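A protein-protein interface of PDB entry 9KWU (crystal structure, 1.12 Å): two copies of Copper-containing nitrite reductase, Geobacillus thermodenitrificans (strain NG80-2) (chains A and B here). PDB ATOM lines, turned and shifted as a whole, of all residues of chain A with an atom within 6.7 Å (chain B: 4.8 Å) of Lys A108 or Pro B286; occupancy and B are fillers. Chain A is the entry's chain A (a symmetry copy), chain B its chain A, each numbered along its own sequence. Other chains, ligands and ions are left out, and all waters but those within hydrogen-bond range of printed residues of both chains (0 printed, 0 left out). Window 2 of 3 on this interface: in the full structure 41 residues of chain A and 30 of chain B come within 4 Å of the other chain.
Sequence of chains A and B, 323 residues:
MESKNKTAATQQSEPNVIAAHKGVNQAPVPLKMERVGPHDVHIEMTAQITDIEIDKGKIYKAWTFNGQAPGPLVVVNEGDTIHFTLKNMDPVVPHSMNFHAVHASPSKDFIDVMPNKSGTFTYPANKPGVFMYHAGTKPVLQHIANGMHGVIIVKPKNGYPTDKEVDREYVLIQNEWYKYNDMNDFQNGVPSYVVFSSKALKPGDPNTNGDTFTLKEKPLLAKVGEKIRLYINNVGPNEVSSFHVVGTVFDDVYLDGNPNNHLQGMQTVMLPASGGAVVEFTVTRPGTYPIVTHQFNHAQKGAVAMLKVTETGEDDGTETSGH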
ATOM      1  N   ALA A 104      21.335  -0.392 -22.629  1.00  0.00           N
ATOM      2  CA  ALA A 104      22.369  -0.905 -23.517  1.00  0.00           C
ATOM      3  C   ALA A 104      23.266   0.239 -23.960  1.00  0.00           C
ATOM      4  O   ALA A 104      22.894   1.411 -23.871  1.00  0.00           O
ATOM      5  CB  ALA A 104      21.755  -1.576 -24.750  1.00  0.00           C
ATOM      6  N   SER A 105      24.463  -0.116 -24.445  1.00  0.00           N
ATOM      7  CA  SER A 105      25.347   0.845 -25.096  1.00  0.00           C
ATOM      8  C   SER A 105      24.939   0.934 -26.561  1.00  0.00           C
ATOM      9  O   SER A 105      25.139  -0.037 -27.300  1.00  0.00           O
ATOM     10  CB  SER A 105      26.790   0.376 -25.007  1.00  0.00           C
ATOM     11  OG  SER A 105      27.587   1.115 -25.924  1.00  0.00           O
ATOM     12  N   PRO A 106      24.399   2.054 -27.043  1.00  0.00           N
ATOM     13  CA  PRO A 106      23.938   2.051 -28.445  1.00  0.00           C
ATOM     14  C   PRO A 106      25.049   1.781 -29.447  1.00  0.00           C
ATOM     15  O   PRO A 106      24.831   1.084 -30.446  1.00  0.00           O
ATOM     16  CB  PRO A 106      23.291   3.430 -28.590  1.00  0.00           C
ATOM     17  CG  PRO A 106      22.807   3.723 -27.204  1.00  0.00           C
ATOM     18  CD  PRO A 106      23.949   3.262 -26.332  1.00  0.00           C
ATOM     19  N   SER A 107      26.252   2.289 -29.185  1.00  0.00           N
ATOM     20  CA  SER A 107      27.359   2.158 -30.126  1.00  0.00           C
ATOM     21  C   SER A 107      28.055   0.802 -30.066  1.00  0.00           C
ATOM     22  O   SER A 107      28.923   0.536 -30.901  1.00  0.00           O
ATOM     23  CB  SER A 107      28.369   3.285 -29.889  1.00  0.00           C
ATOM     24  OG  SER A 107      28.762   3.325 -28.537  1.00  0.00           O
ATOM     25  N   LYS A 108      27.706  -0.053 -29.109  1.00  0.00           N
ATOM     26  CA  LYS A 108      28.204  -1.425 -29.042  1.00  0.00           C
ATOM     27  C   LYS A 108      27.112  -2.454 -29.284  1.00  0.00           C
ATOM     28  O   LYS A 108      27.347  -3.458 -29.964  1.00  0.00           O
ATOM     29  CB  LYS A 108      28.830  -1.679 -27.663  1.00  0.00           C
ATOM     30  CG  LYS A 108      30.035  -0.802 -27.359  1.00  0.00           C
ATOM     31  CD  LYS A 108      30.527  -0.964 -25.923  1.00  0.00           C
ATOM     32  CE  LYS A 108      31.438  -2.168 -25.764  1.00  0.00           C
ATOM     33  NZ  LYS A 108      31.945  -2.278 -24.362  1.00  0.00           N
ATOM     34  N   ASP A 109      25.910  -2.199 -28.769  1.00  0.00           N
ATOM     35  CA  ASP A 109      24.855  -3.200 -28.710  1.00  0.00           C
ATOM     36  C   ASP A 109      23.750  -3.032 -29.741  1.00  0.00           C
ATOM     37  O   ASP A 109      22.995  -3.985 -29.957  1.00  0.00           O
ATOM     38  CB  ASP A 109      24.210  -3.171 -27.317  1.00  0.00           C
ATOM     39  CG  ASP A 109      25.192  -3.470 -26.189  1.00  0.00           C
ATOM     40  OD1 ASP A 109      26.086  -4.334 -26.365  1.00  0.00           O
ATOM     41  OD2 ASP A 109      25.045  -2.840 -25.107  1.00  0.00           O
ATOM     42  N   PHE A 110      23.609  -1.846 -30.336  1.00  0.00           N
ATOM     43  CA  PHE A 110      22.607  -1.570 -31.353  1.00  0.00           C
ATOM     44  C   PHE A 110      23.286  -1.343 -32.708  1.00  0.00           C
ATOM     45  O   PHE A 110      22.861  -0.505 -33.506  1.00  0.00           O
ATOM     46  CB  PHE A 110      21.755  -0.342 -31.012  1.00  0.00           C
ATOM     47  CG  PHE A 110      20.902  -0.425 -29.746  1.00  0.00           C
ATOM     48  CD1 PHE A 110      20.624  -1.612 -29.075  1.00  0.00           C
ATOM     49  CD2 PHE A 110      20.310   0.740 -29.279  1.00  0.00           C
ATOM     50  CE1 PHE A 110      19.784  -1.610 -27.953  1.00  0.00           C
ATOM     51  CE2 PHE A 110      19.489   0.743 -28.176  1.00  0.00           C
ATOM     52  CZ  PHE A 110      19.212  -0.426 -27.516  1.00  0.00           C
ATOM     53  N   ILE A 111      24.328  -2.097 -32.999  1.00  0.00           N
ATOM     54  CA  ILE A 111      25.139  -1.867 -34.188  1.00  0.00           C
ATOM     55  C   ILE A 111      24.627  -2.660 -35.387  1.00  0.00           C
ATOM     56  O   ILE A 111      23.836  -3.602 -35.282  1.00  0.00           O
ATOM     57  CB  ILE A 111      26.636  -2.134 -33.916  1.00  0.00           C
ATOM     58  CG1 ILE A 111      26.835  -3.603 -33.554  1.00  0.00           C
ATOM     59  CG2 ILE A 111      27.143  -1.187 -32.835  1.00  0.00           C
ATOM     60  CD1 ILE A 111      28.298  -4.008 -33.482  1.00  0.00           C
ATOM     61  N   PHE A 121      23.397  -9.754 -29.512  1.00  0.00           N
ATOM     62  CA  PHE A 121      23.533  -8.637 -28.587  1.00  0.00           C
ATOM     63  C   PHE A 121      22.718  -8.958 -27.347  1.00  0.00           C
ATOM     64  O   PHE A 121      21.589  -9.440 -27.463  1.00  0.00           O
ATOM     65  CB  PHE A 121      22.973  -7.378 -29.264  1.00  0.00           C
ATOM     66  CG  PHE A 121      23.510  -7.176 -30.647  1.00  0.00           C
ATOM     67  CD1 PHE A 121      24.793  -6.697 -30.837  1.00  0.00           C
ATOM     68  CD2 PHE A 121      22.769  -7.534 -31.760  1.00  0.00           C
ATOM     69  CE1 PHE A 121      25.312  -6.542 -32.105  1.00  0.00           C
ATOM     70  CE2 PHE A 121      23.287  -7.375 -33.034  1.00  0.00           C
ATOM     71  CZ  PHE A 121      24.556  -6.877 -33.201  1.00  0.00           C
ATOM     72  N   VAL B 224      30.369   5.885 -16.869  1.00  0.00           N
ATOM     73  CA  VAL B 224      29.611   4.640 -16.767  1.00  0.00           C
ATOM     74  C   VAL B 224      28.979   4.515 -15.389  1.00  0.00           C
ATOM     75  O   VAL B 224      29.642   4.695 -14.361  1.00  0.00           O
ATOM     76  CB  VAL B 224      30.517   3.428 -17.067  1.00  0.00           C
ATOM     77  CG1 VAL B 224      29.757   2.131 -16.817  1.00  0.00           C
ATOM     78  CG2 VAL B 224      31.026   3.457 -18.495  1.00  0.00           C
ATOM     79  N   THR B 284      24.367   2.634 -18.306  1.00  0.00           N
ATOM     80  CA  THR B 284      24.945   1.464 -17.657  1.00  0.00           C
ATOM     81  C   THR B 284      26.228   0.954 -18.297  1.00  0.00           C
ATOM     82  O   THR B 284      26.916   0.146 -17.668  1.00  0.00           O
ATOM     83  CB  THR B 284      23.941   0.303 -17.660  1.00  0.00           C
ATOM     84  OG1 THR B 284      23.661  -0.059 -19.019  1.00  0.00           O
ATOM     85  CG2 THR B 284      22.653   0.684 -16.938  1.00  0.00           C
ATOM     86  N   ARG B 285      26.545   1.369 -19.519  1.00  0.00           N
ATOM     87  CA  ARG B 285      27.646   0.815 -20.294  1.00  0.00           C
ATOM     88  C   ARG B 285      28.396   1.920 -21.022  1.00  0.00           C
ATOM     89  O   ARG B 285      27.812   2.957 -21.366  1.00  0.00           O
ATOM     90  CB  ARG B 285      27.122  -0.191 -21.335  1.00  0.00           C
ATOM     91  CG  ARG B 285      26.578  -1.459 -20.720  1.00  0.00           C
ATOM     92  CD  ARG B 285      25.948  -2.387 -21.731  1.00  0.00           C
ATOM     93  NE  ARG B 285      25.439  -3.581 -21.065  1.00  0.00           N
ATOM     94  CZ  ARG B 285      24.852  -4.606 -21.664  1.00  0.00           C
ATOM     95  NH1 ARG B 285      24.661  -4.628 -22.972  1.00  0.00           N
ATOM     96  NH2 ARG B 285      24.424  -5.622 -20.924  1.00  0.00           N
ATOM     97  N   PRO B 286      29.687   1.726 -21.277  1.00  0.00           N
ATOM     98  CA  PRO B 286      30.413   2.718 -22.077  1.00  0.00           C
ATOM     99  C   PRO B 286      29.880   2.755 -23.501  1.00  0.00           C
ATOM    100  O   PRO B 286      29.482   1.728 -24.065  1.00  0.00           O
ATOM    101  CB  PRO B 286      31.862   2.217 -22.027  1.00  0.00           C
ATOM    102  CG  PRO B 286      31.731   0.744 -21.799  1.00  0.00           C
ATOM    103  CD  PRO B 286      30.531   0.563 -20.930  1.00  0.00           C
ATOM    104  N   GLY B 287      29.909   3.946 -24.086  1.00  0.00           N
ATOM    105  CA  GLY B 287      29.542   4.122 -25.472  1.00  0.00           C
ATOM    106  C   GLY B 287      28.955   5.499 -25.703  1.00  0.00           C
ATOM    107  O   GLY B 287      28.943   6.354 -24.814  1.00  0.00           O
ATOM    108  N   THR B 288      28.470   5.706 -26.922  1.00  0.00           N
ATOM    109  CA  THR B 288      27.820   6.951 -27.301  1.00  0.00           C
ATOM    110  C   THR B 288      26.320   6.718 -27.433  1.00  0.00           C
ATOM    111  O   THR B 288      25.883   5.775 -28.104  1.00  0.00           O
ATOM    112  CB  THR B 288      28.435   7.535 -28.571  1.00  0.00           C
ATOM    113  OG1 THR B 288      29.813   7.824 -28.315  1.00  0.00           O
ATOM    114  CG2 THR B 288      27.739   8.821 -28.964  1.00  0.00           C
ATOM    115  N   TYR B 289      25.543   7.576 -26.763  1.00  0.00           N
ATOM    116  CA  TYR B 289      24.099   7.458 -26.625  1.00  0.00           C
ATOM    117  C   TYR B 289      23.436   8.627 -27.343  1.00  0.00           C
ATOM    118  O   TYR B 289      23.551   9.780 -26.879  1.00  0.00           O
ATOM    119  CB  TYR B 289      23.694   7.494 -25.150  1.00  0.00           C
ATOM    120  CG  TYR B 289      24.120   6.314 -24.291  1.00  0.00           C
ATOM    121  CD1 TYR B 289      25.462   6.036 -24.039  1.00  0.00           C
ATOM    122  CD2 TYR B 289      23.167   5.498 -23.702  1.00  0.00           C
ATOM    123  CE1 TYR B 289      25.830   4.965 -23.243  1.00  0.00           C
ATOM    124  CE2 TYR B 289      23.525   4.433 -22.901  1.00  0.00           C
ATOM    125  CZ  TYR B 289      24.863   4.167 -22.674  1.00  0.00           C
ATOM    126  OH  TYR B 289      25.197   3.100 -21.868  1.00  0.00           O
ATOM    127  N   VAL B 309      29.711   8.311 -22.968  1.00  0.00           N
ATOM    128  CA  VAL B 309      29.832   7.734 -21.639  1.00  0.00           C
ATOM    129  C   VAL B 309      31.117   6.915 -21.604  1.00  0.00           C
ATOM    130  O   VAL B 309      31.282   5.953 -22.366  1.00  0.00           O
ATOM    131  CB  VAL B 309      28.605   6.866 -21.316  1.00  0.00           C
ATOM    132  CG1 VAL B 309      28.712   6.245 -19.943  1.00  0.00           C
ATOM    133  CG2 VAL B 309      27.338   7.695 -21.452  1.00  0.00           C
ATOM    134  N   GLU B 311      34.609   5.279 -19.141  1.00  0.00           N
ATOM    135  CA  GLU B 311      34.908   4.711 -17.833  1.00  0.00           C
ATOM    136  C   GLU B 311      35.296   5.785 -16.814  1.00  0.00           C
ATOM    137  O   GLU B 311      35.077   5.596 -15.614  1.00  0.00           O
ATOM    138  CB  GLU B 311      35.958   3.609 -17.952  1.00  0.00           C
ATOM    139  CG  GLU B 311      35.463   2.355 -18.692  1.00  0.00           C
ATOM    140  CD  GLU B 311      34.308   1.619 -18.000  1.00  0.00           C
ATOM    141  OE1 GLU B 311      34.068   1.847 -16.794  1.00  0.00           O
ATOM    142  OE2 GLU B 311      33.649   0.788 -18.665  1.00  0.00           O
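Among the printed residues, pairs that only touch across the chains: Ser A107 with Gly B287 (3.3 Å), Lys A108 with Pro B286 (3.4 Å), Pro A106 with Thr B288 (3.5 Å), Pro A106 with Tyr B289 (3.5 Å), Ser A105 with Gly B287 (3.6 Å), Ser A105 with Arg B285 (3.7 Å) and Ser A105 with Tyr B289 (3.9 Å).
NH1 of Arg B285 lies within salt-bridge range of OD2 of Asp A109 (2.8 Å). The backbone carbonyl oxygen of Pro B286 sits at hydrogen-bond distance from the side-chain hydroxyl of Ser A105, 2.7 Å away. N of Thr B288 lies within hydrogen-bond range of OG of Ser A107 (2.9 Å). The backbone carbonyl oxygen of Ala A104 sits close to the side-chain hydroxyl of Tyr B289.
No position is printed for both chains.
Of the 9 printed residues of chain B, 5 touch a printed residue of chain A. Of the 9 printed residues of chain A, 6 touch a printed residue of chain B. Printed residues of chain A that touch a printed residue of chain B: Ala A104, Ser A105, Pro A106, Ser A107, Lys A108 and Asp A109. Hydrophobic or aromatic side chains of chain A within 4 Å of the printed part of chain B: Pro A106. Among the printed residues, Asp or Glu carboxylates within 4 Å of a Lys or Arg side-chain nitrogen of the other chain: Asp A109 with Arg B285.
O of Arg B285 lies within hydrogen-bond range of OH of Tyr B289 (2.7 Å). The backbone carbonyl oxygen of Gly B287 sits at hydrogen-bond distance from the backbone NH of Val B309 (2.8 Å). The backbone NH (N) of Lys A108 is in hydrogen-bond range of the side-chain hydroxyl (OG) of Ser A105. N of Ser A105 is in hydrogen-bond range of OD2 of Asp A109 (2.9 Å).
Of the printed residues of chain B, Ala A104 touches Tyr B289. Printed residues of chain B within 4 Å of Lys A108: Pro B286. Of the printed residues of chain A, Gly B287 touches Ser A105 (3.6 Å) and Ser A107 (3.3 Å). Val B309 touches none of the printed residues of chain A. The nearest printed residue of chain B that does not touch Pro A106 is Gly B287 (5.5 Å).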
